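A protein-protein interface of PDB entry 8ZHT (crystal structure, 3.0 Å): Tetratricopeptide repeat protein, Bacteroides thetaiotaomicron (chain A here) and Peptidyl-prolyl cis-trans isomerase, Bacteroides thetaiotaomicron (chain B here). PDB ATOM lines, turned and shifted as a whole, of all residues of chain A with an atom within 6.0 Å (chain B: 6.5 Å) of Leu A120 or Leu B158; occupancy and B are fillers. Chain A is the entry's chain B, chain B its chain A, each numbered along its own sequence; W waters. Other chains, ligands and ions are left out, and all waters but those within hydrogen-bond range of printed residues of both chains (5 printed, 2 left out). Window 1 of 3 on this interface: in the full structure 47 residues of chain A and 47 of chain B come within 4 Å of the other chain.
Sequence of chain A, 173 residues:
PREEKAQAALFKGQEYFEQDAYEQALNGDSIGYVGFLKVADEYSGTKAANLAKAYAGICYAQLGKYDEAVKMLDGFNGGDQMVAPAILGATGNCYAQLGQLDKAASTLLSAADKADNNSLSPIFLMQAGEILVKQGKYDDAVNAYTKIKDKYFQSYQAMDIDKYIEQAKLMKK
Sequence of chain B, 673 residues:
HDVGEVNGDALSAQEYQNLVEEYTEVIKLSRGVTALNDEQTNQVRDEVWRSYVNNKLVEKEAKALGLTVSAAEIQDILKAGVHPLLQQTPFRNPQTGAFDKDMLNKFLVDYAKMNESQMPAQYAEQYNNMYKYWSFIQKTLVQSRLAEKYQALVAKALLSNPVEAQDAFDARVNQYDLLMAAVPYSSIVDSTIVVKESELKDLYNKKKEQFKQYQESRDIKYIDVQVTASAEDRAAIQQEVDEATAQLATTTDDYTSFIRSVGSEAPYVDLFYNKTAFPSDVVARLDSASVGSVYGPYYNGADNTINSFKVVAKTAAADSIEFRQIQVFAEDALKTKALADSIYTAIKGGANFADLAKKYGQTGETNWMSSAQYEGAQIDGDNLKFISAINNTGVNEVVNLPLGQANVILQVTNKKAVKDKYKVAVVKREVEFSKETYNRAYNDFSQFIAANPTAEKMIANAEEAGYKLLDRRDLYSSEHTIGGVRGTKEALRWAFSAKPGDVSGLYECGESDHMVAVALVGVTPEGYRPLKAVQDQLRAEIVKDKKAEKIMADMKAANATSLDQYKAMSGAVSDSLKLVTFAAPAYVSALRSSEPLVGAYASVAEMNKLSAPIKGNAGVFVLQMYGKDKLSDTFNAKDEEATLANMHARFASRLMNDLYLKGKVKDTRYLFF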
ATOM      1  N   ILE A  58      11.432 -19.219 -19.692  1.00  0.00           N
ATOM      2  CA  ILE A  58      10.955 -18.032 -18.975  1.00  0.00           C
ATOM      3  C   ILE A  58      11.377 -18.093 -17.514  1.00  0.00           C
ATOM      4  O   ILE A  58      11.731 -17.070 -16.916  1.00  0.00           O
ATOM      5  CB  ILE A  58       9.421 -17.889 -19.092  1.00  0.00           C
ATOM      6  CG1 ILE A  58       8.975 -17.704 -20.542  1.00  0.00           C
ATOM      7  CG2 ILE A  58       8.916 -16.718 -18.261  1.00  0.00           C
ATOM      8  CD1 ILE A  58       9.810 -16.688 -21.302  1.00  0.00           C
ATOM      9  N   GLN A  81      -0.163 -17.848 -33.286  1.00  0.00           N
ATOM     10  CA  GLN A  81      -0.130 -16.388 -33.395  1.00  0.00           C
ATOM     11  C   GLN A  81       0.486 -15.713 -32.175  1.00  0.00           C
ATOM     12  O   GLN A  81       1.058 -14.622 -32.299  1.00  0.00           O
ATOM     13  CB  GLN A  81      -1.544 -15.824 -33.559  1.00  0.00           C
ATOM     14  CG  GLN A  81      -2.493 -16.682 -34.342  1.00  0.00           C
ATOM     15  CD  GLN A  81      -3.885 -16.065 -34.393  1.00  0.00           C
ATOM     16  OE1 GLN A  81      -4.037 -14.830 -34.306  1.00  0.00           O
ATOM     17  NE2 GLN A  81      -4.916 -16.923 -34.496  1.00  0.00           N
ATOM     18  N   MET A  82       0.361 -16.321 -30.995  1.00  0.00           N
ATOM     19  CA  MET A  82       0.610 -15.642 -29.726  1.00  0.00           C
ATOM     20  C   MET A  82       1.828 -16.195 -28.986  1.00  0.00           C
ATOM     21  O   MET A  82       2.767 -15.449 -28.698  1.00  0.00           O
ATOM     22  CB  MET A  82      -0.652 -15.761 -28.852  1.00  0.00           C
ATOM     23  CG  MET A  82      -1.807 -14.784 -29.151  1.00  0.00           C
ATOM     24  SD  MET A  82      -1.402 -13.103 -29.683  1.00  0.00           S
ATOM     25  CE  MET A  82      -2.802 -12.703 -30.749  1.00  0.00           C
ATOM     26  N   VAL A  83       1.842 -17.491 -28.667  1.00  0.00           N
ATOM     27  CA  VAL A  83       2.881 -18.019 -27.781  1.00  0.00           C
ATOM     28  C   VAL A  83       4.237 -18.046 -28.479  1.00  0.00           C
ATOM     29  O   VAL A  83       5.237 -17.562 -27.933  1.00  0.00           O
ATOM     30  CB  VAL A  83       2.478 -19.407 -27.251  1.00  0.00           C
ATOM     31  CG1 VAL A  83       3.685 -20.135 -26.688  1.00  0.00           C
ATOM     32  CG2 VAL A  83       1.412 -19.242 -26.193  1.00  0.00           C
ATOM     33  N   PRO A  85       5.573 -16.318 -31.155  1.00  0.00           N
ATOM     34  CA  PRO A  85       6.246 -15.004 -31.240  1.00  0.00           C
ATOM     35  C   PRO A  85       6.649 -14.454 -29.882  1.00  0.00           C
ATOM     36  O   PRO A  85       7.722 -13.859 -29.755  1.00  0.00           O
ATOM     37  CB  PRO A  85       5.212 -14.107 -31.945  1.00  0.00           C
ATOM     38  CG  PRO A  85       4.220 -15.056 -32.579  1.00  0.00           C
ATOM     39  CD  PRO A  85       4.223 -16.293 -31.752  1.00  0.00           C
ATOM     40  N   ALA A  86       5.827 -14.635 -28.850  1.00  0.00           N
ATOM     41  CA  ALA A  86       6.234 -14.143 -27.535  1.00  0.00           C
ATOM     42  C   ALA A  86       7.484 -14.870 -27.036  1.00  0.00           C
ATOM     43  O   ALA A  86       8.353 -14.267 -26.389  1.00  0.00           O
ATOM     44  CB  ALA A  86       5.085 -14.286 -26.548  1.00  0.00           C
ATOM     45  N   ALA A  90      10.831 -13.093 -26.144  1.00  0.00           N
ATOM     46  CA  ALA A  90      11.555 -13.298 -24.891  1.00  0.00           C
ATOM     47  C   ALA A  90      13.028 -13.617 -25.148  1.00  0.00           C
ATOM     48  O   ALA A  90      13.905 -13.148 -24.414  1.00  0.00           O
ATOM     49  CB  ALA A  90      10.895 -14.407 -24.068  1.00  0.00           C
ATOM     50  N   ASN A  93      14.844 -10.436 -25.843  1.00  0.00           N
ATOM     51  CA  ASN A  93      15.053  -9.687 -24.615  1.00  0.00           C
ATOM     52  C   ASN A  93      16.172 -10.287 -23.765  1.00  0.00           C
ATOM     53  O   ASN A  93      16.925  -9.535 -23.133  1.00  0.00           O
ATOM     54  CB  ASN A  93      13.730  -9.589 -23.856  1.00  0.00           C
ATOM     55  CG  ASN A  93      12.832  -8.512 -24.457  1.00  0.00           C
ATOM     56  OD1 ASN A  93      13.246  -7.365 -24.533  1.00  0.00           O
ATOM     57  ND2 ASN A  93      11.648  -8.890 -24.968  1.00  0.00           N
ATOM     58  N   ALA A 112       8.099  -9.687 -34.092  1.00  0.00           N
ATOM     59  CA  ALA A 112       7.016  -8.808 -34.524  1.00  0.00           C
ATOM     60  C   ALA A 112       6.431  -9.250 -35.867  1.00  0.00           C
ATOM     61  O   ALA A 112       5.207  -9.210 -36.063  1.00  0.00           O
ATOM     62  CB  ALA A 112       7.520  -7.361 -34.603  1.00  0.00           C
ATOM     63  N   ALA A 115       4.372 -12.467 -35.245  1.00  0.00           N
ATOM     64  CA  ALA A 115       3.111 -12.238 -34.544  1.00  0.00           C
ATOM     65  C   ALA A 115       2.102 -11.556 -35.461  1.00  0.00           C
ATOM     66  O   ALA A 115       0.953 -11.996 -35.573  1.00  0.00           O
ATOM     67  CB  ALA A 115       3.353 -11.387 -33.291  1.00  0.00           C
ATOM     68  N   ASN A 117       0.332  -8.815 -35.249  1.00  0.00           N
ATOM     69  CA  ASN A 117      -0.950  -8.443 -34.659  1.00  0.00           C
ATOM     70  C   ASN A 117      -0.760  -7.264 -33.714  1.00  0.00           C
ATOM     71  O   ASN A 117       0.359  -6.912 -33.340  1.00  0.00           O
ATOM     72  CB  ASN A 117      -1.620  -9.632 -33.945  1.00  0.00           C
ATOM     73  CG  ASN A 117      -0.728 -10.294 -32.905  1.00  0.00           C
ATOM     74  OD1 ASN A 117      -0.158  -9.625 -32.043  1.00  0.00           O
ATOM     75  ND2 ASN A 117      -0.638 -11.624 -32.958  1.00  0.00           N
ATOM     76  N   ASN A 118      -1.893  -6.667 -33.329  1.00  0.00           N
ATOM     77  CA  ASN A 118      -1.902  -5.453 -32.521  1.00  0.00           C
ATOM     78  C   ASN A 118      -1.476  -5.705 -31.080  1.00  0.00           C
ATOM     79  O   ASN A 118      -1.001  -4.780 -30.422  1.00  0.00           O
ATOM     80  CB  ASN A 118      -3.302  -4.824 -32.520  1.00  0.00           C
ATOM     81  CG  ASN A 118      -3.699  -4.257 -33.880  1.00  0.00           C
ATOM     82  OD1 ASN A 118      -2.960  -3.485 -34.494  1.00  0.00           O
ATOM     83  ND2 ASN A 118      -4.874  -4.648 -34.355  1.00  0.00           N
ATOM     84  N   SER A 119      -1.665  -6.922 -30.553  1.00  0.00           N
ATOM     85  CA  SER A 119      -1.327  -7.174 -29.148  1.00  0.00           C
ATOM     86  C   SER A 119       0.161  -7.381 -28.934  1.00  0.00           C
ATOM     87  O   SER A 119       0.690  -6.953 -27.908  1.00  0.00           O
ATOM     88  CB  SER A 119      -2.078  -8.386 -28.593  1.00  0.00           C
ATOM     89  OG  SER A 119      -3.440  -8.383 -28.988  1.00  0.00           O
ATOM     90  N   LEU A 120       0.858  -8.022 -29.871  1.00  0.00           N
ATOM     91  CA  LEU A 120       2.263  -8.361 -29.663  1.00  0.00           C
ATOM     92  C   LEU A 120       3.237  -7.619 -30.560  1.00  0.00           C
ATOM     93  O   LEU A 120       4.310  -7.233 -30.097  1.00  0.00           O
ATOM     94  CB  LEU A 120       2.490  -9.866 -29.849  1.00  0.00           C
ATOM     95  CG  LEU A 120       1.750 -10.752 -28.857  1.00  0.00           C
ATOM     96  CD1 LEU A 120       2.175 -12.226 -29.040  1.00  0.00           C
ATOM     97  CD2 LEU A 120       2.003 -10.272 -27.432  1.00  0.00           C
ATOM     98  N   SER A 121       2.950  -7.470 -31.848  1.00  0.00           N
ATOM     99  CA  SER A 121       3.920  -6.816 -32.722  1.00  0.00           C
ATOM    100  C   SER A 121       4.382  -5.461 -32.213  1.00  0.00           C
ATOM    101  O   SER A 121       5.601  -5.203 -32.259  1.00  0.00           O
ATOM    102  CB  SER A 121       3.345  -6.685 -34.142  1.00  0.00           C
ATOM    103  OG  SER A 121       3.131  -7.969 -34.678  1.00  0.00           O
ATOM    104  N   PRO A 122       3.511  -4.567 -31.711  1.00  0.00           N
ATOM    105  CA  PRO A 122       4.012  -3.256 -31.253  1.00  0.00           C
ATOM    106  C   PRO A 122       4.918  -3.345 -30.039  1.00  0.00           C
ATOM    107  O   PRO A 122       5.816  -2.504 -29.895  1.00  0.00           O
ATOM    108  CB  PRO A 122       2.726  -2.462 -30.941  1.00  0.00           C
ATOM    109  CG  PRO A 122       1.636  -3.178 -31.622  1.00  0.00           C
ATOM    110  CD  PRO A 122       2.036  -4.626 -31.674  1.00  0.00           C
ATOM    111  N   ILE A 123       4.709  -4.324 -29.153  1.00  0.00           N
ATOM    112  CA  ILE A 123       5.602  -4.482 -28.007  1.00  0.00           C
ATOM    113  C   ILE A 123       7.027  -4.735 -28.486  1.00  0.00           C
ATOM    114  O   ILE A 123       7.983  -4.075 -28.050  1.00  0.00           O
ATOM    115  CB  ILE A 123       5.118  -5.624 -27.095  1.00  0.00           C
ATOM    116  CG1 ILE A 123       3.768  -5.277 -26.466  1.00  0.00           C
ATOM    117  CG2 ILE A 123       6.178  -5.920 -26.011  1.00  0.00           C
ATOM    118  CD1 ILE A 123       3.106  -6.435 -25.723  1.00  0.00           C
ATOM    119  N   PHE A 124       7.180  -5.685 -29.416  1.00  0.00           N
ATOM    120  CA  PHE A 124       8.510  -6.040 -29.913  1.00  0.00           C
ATOM    121  C   PHE A 124       9.095  -4.944 -30.789  1.00  0.00           C
ATOM    122  O   PHE A 124      10.309  -4.710 -30.742  1.00  0.00           O
ATOM    123  CB  PHE A 124       8.442  -7.377 -30.671  1.00  0.00           C
ATOM    124  CG  PHE A 124       7.835  -8.476 -29.865  1.00  0.00           C
ATOM    125  CD1 PHE A 124       8.135  -8.598 -28.515  1.00  0.00           C
ATOM    126  CD2 PHE A 124       6.928  -9.364 -30.434  1.00  0.00           C
ATOM    127  CE1 PHE A 124       7.572  -9.597 -27.756  1.00  0.00           C
ATOM    128  CE2 PHE A 124       6.346 -10.386 -29.659  1.00  0.00           C
ATOM    129  CZ  PHE A 124       6.670 -10.502 -28.332  1.00  0.00           C
ATOM    130  N   LEU A 125       8.252  -4.242 -31.563  1.00  0.00           N
ATOM    131  CA  LEU A 125       8.764  -3.160 -32.399  1.00  0.00           C
ATOM    132  C   LEU A 125       9.291  -2.016 -31.547  1.00  0.00           C
ATOM    133  O   LEU A 125      10.338  -1.443 -31.868  1.00  0.00           O
ATOM    134  CB  LEU A 125       7.684  -2.670 -33.376  1.00  0.00           C
ATOM    135  CG  LEU A 125       7.406  -3.615 -34.561  1.00  0.00           C
ATOM    136  CD1 LEU A 125       6.083  -3.311 -35.216  1.00  0.00           C
ATOM    137  CD2 LEU A 125       8.514  -3.583 -35.603  1.00  0.00           C
ATOM    138  N   GLN A 127      10.544  -2.316 -28.487  1.00  0.00           N
ATOM    139  CA  GLN A 127      11.791  -2.767 -27.884  1.00  0.00           C
ATOM    140  C   GLN A 127      12.919  -2.770 -28.900  1.00  0.00           C
ATOM    141  O   GLN A 127      14.049  -2.377 -28.584  1.00  0.00           O
ATOM    142  CB  GLN A 127      11.591  -4.152 -27.276  1.00  0.00           C
ATOM    143  CG  GLN A 127      10.655  -4.111 -26.082  1.00  0.00           C
ATOM    144  CD  GLN A 127      10.498  -5.473 -25.427  1.00  0.00           C
ATOM    145  OE1 GLN A 127      10.152  -6.458 -26.078  1.00  0.00           O
ATOM    146  NE2 GLN A 127      10.751  -5.528 -24.140  1.00  0.00           N
ATOM    147  N   LEU B 153       0.744 -17.714 -20.224  1.00  0.00           N
ATOM    148  CA  LEU B 153       1.978 -18.070 -20.902  1.00  0.00           C
ATOM    149  C   LEU B 153       2.407 -16.942 -21.826  1.00  0.00           C
ATOM    150  O   LEU B 153       3.577 -16.551 -21.829  1.00  0.00           O
ATOM    151  CB  LEU B 153       1.805 -19.387 -21.658  1.00  0.00           C
ATOM    152  CG  LEU B 153       2.966 -19.958 -22.466  1.00  0.00           C
ATOM    153  CD1 LEU B 153       4.288 -19.947 -21.697  1.00  0.00           C
ATOM    154  CD2 LEU B 153       2.614 -21.375 -22.903  1.00  0.00           C
ATOM    155  N   VAL B 154       1.462 -16.368 -22.571  1.00  0.00           N
ATOM    156  CA  VAL B 154       1.771 -15.215 -23.410  1.00  0.00           C
ATOM    157  C   VAL B 154       2.300 -14.073 -22.555  1.00  0.00           C
ATOM    158  O   VAL B 154       3.397 -13.556 -22.799  1.00  0.00           O
ATOM    159  CB  VAL B 154       0.533 -14.788 -24.223  1.00  0.00           C
ATOM    160  CG1 VAL B 154       0.836 -13.545 -25.044  1.00  0.00           C
ATOM    161  CG2 VAL B 154       0.051 -15.937 -25.113  1.00  0.00           C
ATOM    162  N   ALA B 155       1.552 -13.712 -21.498  1.00  0.00           N
ATOM    163  CA  ALA B 155       1.851 -12.513 -20.710  1.00  0.00           C
ATOM    164  C   ALA B 155       3.221 -12.587 -20.056  1.00  0.00           C
ATOM    165  O   ALA B 155       3.983 -11.609 -20.069  1.00  0.00           O
ATOM    166  CB  ALA B 155       0.783 -12.303 -19.630  1.00  0.00           C
ATOM    167  N   LYS B 156       3.543 -13.729 -19.453  1.00  0.00           N
ATOM    168  CA  LYS B 156       4.784 -13.850 -18.701  1.00  0.00           C
ATOM    169  C   LYS B 156       6.009 -13.944 -19.598  1.00  0.00           C
ATOM    170  O   LYS B 156       7.118 -13.660 -19.140  1.00  0.00           O
ATOM    171  CB  LYS B 156       4.691 -15.057 -17.766  1.00  0.00           C
ATOM    172  CG  LYS B 156       3.770 -14.771 -16.559  1.00  0.00           C
ATOM    173  CD  LYS B 156       4.028 -15.721 -15.408  1.00  0.00           C
ATOM    174  CE  LYS B 156       3.410 -15.203 -14.113  1.00  0.00           C
ATOM    175  NZ  LYS B 156       3.379 -13.716 -14.053  1.00  0.00           N
ATOM    176  N   ALA B 157       5.830 -14.307 -20.867  1.00  0.00           N
ATOM    177  CA  ALA B 157       6.904 -14.279 -21.840  1.00  0.00           C
ATOM    178  C   ALA B 157       7.233 -12.871 -22.327  1.00  0.00           C
ATOM    179  O   ALA B 157       8.162 -12.727 -23.128  1.00  0.00           O
ATOM    180  CB  ALA B 157       6.537 -15.145 -23.050  1.00  0.00           C
ATOM    181  N   LEU B 158       6.490 -11.837 -21.902  1.00  0.00           N
ATOM    182  CA  LEU B 158       6.703 -10.479 -22.429  1.00  0.00           C
ATOM    183  C   LEU B 158       7.679  -9.736 -21.524  1.00  0.00           C
ATOM    184  O   LEU B 158       7.330  -8.816 -20.786  1.00  0.00           O
ATOM    185  CB  LEU B 158       5.382  -9.739 -22.570  1.00  0.00           C
ATOM    186  CG  LEU B 158       4.380 -10.461 -23.485  1.00  0.00           C
ATOM    187  CD1 LEU B 158       3.040  -9.787 -23.411  1.00  0.00           C
ATOM    188  CD2 LEU B 158       4.872 -10.512 -24.941  1.00  0.00           C
ATOM    189  N   LEU B 159       8.933 -10.175 -21.594  1.00  0.00           N
ATOM    190  CA  LEU B 159       9.985  -9.661 -20.733  1.00  0.00           C
ATOM    191  C   LEU B 159      10.356  -8.229 -21.099  1.00  0.00           C
ATOM    192  O   LEU B 159      10.089  -7.736 -22.204  1.00  0.00           O
ATOM    193  CB  LEU B 159      11.246 -10.516 -20.842  1.00  0.00           C
ATOM    194  CG  LEU B 159      11.126 -12.034 -20.717  1.00  0.00           C
ATOM    195  CD1 LEU B 159      12.533 -12.611 -20.703  1.00  0.00           C
ATOM    196  CD2 LEU B 159      10.356 -12.413 -19.457  1.00  0.00           C
ATOM    197  N   SER B 160      11.033  -7.584 -20.169  1.00  0.00           N
ATOM    198  CA  SER B 160      11.691  -6.321 -20.439  1.00  0.00           C
ATOM    199  C   SER B 160      13.189  -6.565 -20.632  1.00  0.00           C
ATOM    200  O   SER B 160      13.647  -7.704 -20.743  1.00  0.00           O
ATOM    201  CB  SER B 160      11.409  -5.334 -19.311  1.00  0.00           C
ATOM    202  OG  SER B 160      11.839  -4.048 -19.707  1.00  0.00           O
ATOM    203  N   GLU B 641      12.163  -2.994 -14.896  1.00  0.00           N
ATOM    204  CA  GLU B 641      11.776  -4.077 -15.805  1.00  0.00           C
ATOM    205  C   GLU B 641      10.480  -4.745 -15.377  1.00  0.00           C
ATOM    206  O   GLU B 641       9.679  -5.154 -16.229  1.00  0.00           O
ATOM    207  CB  GLU B 641      12.891  -5.116 -15.901  1.00  0.00           C
ATOM    208  CG  GLU B 641      14.180  -4.535 -16.471  1.00  0.00           C
ATOM    209  CD  GLU B 641      15.309  -5.558 -16.620  1.00  0.00           C
ATOM    210  OE1 GLU B 641      15.023  -6.784 -16.638  1.00  0.00           O
ATOM    211  OE2 GLU B 641      16.483  -5.116 -16.745  1.00  0.00           O
ATOM    212  N   LEU B 644       7.695  -2.525 -16.554  1.00  0.00           N
ATOM    213  CA  LEU B 644       7.511  -2.624 -17.996  1.00  0.00           C
ATOM    214  C   LEU B 644       6.893  -3.965 -18.385  1.00  0.00           C
ATOM    215  O   LEU B 644       5.976  -4.008 -19.225  1.00  0.00           O
ATOM    216  CB  LEU B 644       8.849  -2.400 -18.700  1.00  0.00           C
ATOM    217  CG  LEU B 644       9.330  -0.949 -18.603  1.00  0.00           C
ATOM    218  CD1 LEU B 644      10.805  -0.841 -18.911  1.00  0.00           C
ATOM    219  CD2 LEU B 644       8.540  -0.053 -19.572  1.00  0.00           C
ATOM    220  N   ALA B 645       7.353  -5.064 -17.760  1.00  0.00           N
ATOM    221  CA  ALA B 645       6.768  -6.380 -18.028  1.00  0.00           C
ATOM    222  C   ALA B 645       5.266  -6.383 -17.755  1.00  0.00           C
ATOM    223  O   ALA B 645       4.480  -6.857 -18.585  1.00  0.00           O
ATOM    224  CB  ALA B 645       7.486  -7.468 -17.205  1.00  0.00           C
ATOM    225  N   ASN B 646       4.835  -5.807 -16.620  1.00  0.00           N
ATOM    226  CA  ASN B 646       3.398  -5.736 -16.336  1.00  0.00           C
ATOM    227  C   ASN B 646       2.661  -4.834 -17.320  1.00  0.00           C
ATOM    228  O   ASN B 646       1.537  -5.148 -17.733  1.00  0.00           O
ATOM    229  CB  ASN B 646       3.141  -5.268 -14.902  1.00  0.00           C
ATOM    230  CG  ASN B 646       3.569  -6.297 -13.881  1.00  0.00           C
ATOM    231  OD1 ASN B 646       4.378  -6.010 -13.000  1.00  0.00           O
ATOM    232  ND2 ASN B 646       3.080  -7.530 -14.037  1.00  0.00           N
ATOM    233  N   HIS B 648       3.522  -4.526 -20.451  1.00  0.00           N
ATOM    234  CA  HIS B 648       3.353  -5.352 -21.648  1.00  0.00           C
ATOM    235  C   HIS B 648       2.133  -6.261 -21.528  1.00  0.00           C
ATOM    236  O   HIS B 648       1.351  -6.385 -22.477  1.00  0.00           O
ATOM    237  CB  HIS B 648       4.602  -6.186 -21.925  1.00  0.00           C
ATOM    238  CG  HIS B 648       5.837  -5.374 -22.136  1.00  0.00           C
ATOM    239  ND1 HIS B 648       7.098  -5.846 -21.836  1.00  0.00           N
ATOM    240  CD2 HIS B 648       6.003  -4.112 -22.606  1.00  0.00           C
ATOM    241  CE1 HIS B 648       7.987  -4.910 -22.127  1.00  0.00           C
ATOM    242  NE2 HIS B 648       7.348  -3.851 -22.599  1.00  0.00           N
ATOM    243  N   ALA B 649       1.937  -6.871 -20.353  1.00  0.00           N
ATOM    244  CA  ALA B 649       0.789  -7.756 -20.131  1.00  0.00           C
ATOM    245  C   ALA B 649      -0.525  -7.005 -20.303  1.00  0.00           C
ATOM    246  O   ALA B 649      -1.418  -7.456 -21.032  1.00  0.00           O
ATOM    247  CB  ALA B 649       0.862  -8.393 -18.733  1.00  0.00           C
ATOM    248  N   PHE B 651      -0.979  -4.256 -22.039  1.00  0.00           N
ATOM    249  CA  PHE B 651      -1.142  -3.849 -23.437  1.00  0.00           C
ATOM    250  C   PHE B 651      -1.580  -5.008 -24.321  1.00  0.00           C
ATOM    251  O   PHE B 651      -2.175  -4.779 -25.382  1.00  0.00           O
ATOM    252  CB  PHE B 651       0.162  -3.275 -24.006  1.00  0.00           C
ATOM    253  CG  PHE B 651       0.424  -1.816 -23.660  1.00  0.00           C
ATOM    254  CD1 PHE B 651      -0.496  -1.060 -22.940  1.00  0.00           C
ATOM    255  CD2 PHE B 651       1.625  -1.212 -24.045  1.00  0.00           C
ATOM    256  CE1 PHE B 651      -0.237   0.282 -22.628  1.00  0.00           C
ATOM    257  CE2 PHE B 651       1.894   0.126 -23.739  1.00  0.00           C
ATOM    258  CZ  PHE B 651       0.962   0.874 -23.031  1.00  0.00           C
ATOM    259  N   ALA B 652      -1.262  -6.248 -23.938  1.00  0.00           N
ATOM    260  CA  ALA B 652      -1.638  -7.427 -24.715  1.00  0.00           C
ATOM    261  C   ALA B 652      -2.890  -8.124 -24.191  1.00  0.00           C
ATOM    262  O   ALA B 652      -3.250  -9.192 -24.704  1.00  0.00           O
ATOM    263  CB  ALA B 652      -0.482  -8.433 -24.752  1.00  0.00           C
ATOM    264  N   LEU B 655      -5.873  -9.796 -26.466  1.00  0.00           N
ATOM    265  CA  LEU B 655      -5.444 -10.662 -27.557  1.00  0.00           C
ATOM    266  C   LEU B 655      -6.587 -11.513 -28.110  1.00  0.00           C
ATOM    267  O   LEU B 655      -6.537 -11.892 -29.280  1.00  0.00           O
ATOM    268  CB  LEU B 655      -4.258 -11.531 -27.110  1.00  0.00           C
ATOM    269  CG  LEU B 655      -4.387 -12.505 -25.932  1.00  0.00           C
ATOM    270  CD1 LEU B 655      -5.171 -13.749 -26.324  1.00  0.00           C
ATOM    271  CD2 LEU B 655      -3.004 -12.892 -25.406  1.00  0.00           C
ATOM    272  N   ASP B 658      -7.619 -10.222 -31.443  1.00  0.00           N
ATOM    273  CA  ASP B 658      -6.790 -10.687 -32.555  1.00  0.00           C
ATOM    274  C   ASP B 658      -7.131 -12.106 -32.958  1.00  0.00           C
ATOM    275  O   ASP B 658      -7.165 -12.417 -34.153  1.00  0.00           O
ATOM    276  CB  ASP B 658      -5.310 -10.608 -32.194  1.00  0.00           C
ATOM    277  CG  ASP B 658      -4.934  -9.270 -31.622  1.00  0.00           C
ATOM    278  OD1 ASP B 658      -5.171  -9.046 -30.411  1.00  0.00           O
ATOM    279  OD2 ASP B 658      -4.404  -8.437 -32.384  1.00  0.00           O
HETATM  280  O   HOH W   1      -1.636  -2.678 -28.117  1.00  0.00           O
HETATM  281  O   HOH W   2      -4.086  -7.464 -34.804  1.00  0.00           O
HETATM  282  O   HOH W   3      -4.283  -6.220 -26.734  1.00  0.00           O
HETATM  283  O   HOH W   4       8.433  -8.141 -24.387  1.00  0.00           O
HETATM  284  O   HOH W   5       7.581  -2.491 -25.747  1.00  0.00           O
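Of the printed residues of chain B, Gln A81 touches Asp B658. Printed residues of chain B within 4 Å of Val A83: Val B154. Of the printed residues of chain B, Ala A86 touches Ala B157. Leu B158 touches just these residues of chain A: Leu A120 (3.8 Å) and Phe A124 (3.8 Å). Of the printed residues of chain A, Leu B159 touches Ala A90, Asn A93 and Gln A127. Glu B641 touches none of the printed residues of chain A. The nearest residue of chain B that does not touch Leu A120 is Ala B652 (4.1 Å). The nearest residue of chain A that does not touch Leu B158 is Ile A123 (4.1 Å). The nearest printed residue of chain B that does not touch Met A82 is Leu B655 (4.1 Å).
Water W2 lies within hydrogen-bond range of the side-chain carboxylate of Asp B658 and the backbone NH of Asn A118. Water W4 lies within hydrogen-bond range of O of Leu B159 (2.8 Å), OE1 of Gln A127 (2.9 Å) and ND2 of Asn A93 (3.4 Å). Water W5 lies within hydrogen-bond range of the backbone carbonyl oxygen (O) of Ile A123 (2.8 Å) and a ring nitrogen (NE2) of His B648 (3.4 Å). Water W3 bridges the backbone carbonyl oxygen (O) of Phe B651 and the side-chain hydroxyl (OG) of Ser A119. Water W1 lies within hydrogen-bond range of the backbone carbonyl oxygen (O) of Asn A118 (3.2 Å) and the backbone carbonyl oxygen (O) of Phe B651 (3.5 Å).
Among the printed residues, pairs that only touch across the chains: Ala A90 with Ala B157, Ser A119 with Leu B655, Asn A117 with Asp B658, Gln A127 with His B648, Met A82 with Asp B658, Ala A86 with Ala B157, Asn A93 with Ser B160, Ile A58 with Lys B156, Ser A119 with Ala B652, Ile A123 with His B648, Val A83 with Val B154, Leu A120 with Leu B158, Met A82 with Val B154, Ile A58 with Ala B157, Phe A124 with Leu B158, Gln A127 with Ser B160, Gln A81 with Asp B658 and Ala A90 with Leu B159.
ND1 of His B648 sits at hydrogen-bond distance from O of Leu B158, at 3.2 Å. The side-chain sulfur of Met A82 lies close to the side-chain amide nitrogen of Asn A117 (3.7 Å). ND2 of Asn A93 sits at hydrogen-bond distance from OE1 of Gln A127. The side-chain amide nitrogen (ND2) of Asn A117 lies within hydrogen-bond range of the backbone carbonyl oxygen (O) of Ala A115 (3.1 Å). OD1 of Asn A117 lies within hydrogen-bond range of N of Leu A120, 2.9 Å away. The side-chain hydroxyl (OG) of Ser A121 lies within hydrogen-bond range of the backbone NH (N) of Asn A117 (3.0 Å).
O of Leu B159 is in hydrogen-bond range of ND2 of Asn A93, 3.4 Å away. O of Leu B159 sits at hydrogen-bond distance from NE2 of Gln A127. N of Asn A118 sits at hydrogen-bond distance from OD2 of Asp B658 (3.2 Å). The side-chain hydroxyl (OG) of Ser A119 lies close to the side-chain carboxylate (OD1) of Asp B658.
Printed residues of chain A that touch a printed residue of chain B: Ile A58, Gln A81, Met A82, Val A83, Ala A86, Ala A90, Asn A93, Asn A117, Asn A118, Ser A119, Leu A120, Ile A123, Phe A124 and Gln A127. Among the printed residues, 22 pairs touch across the chains.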
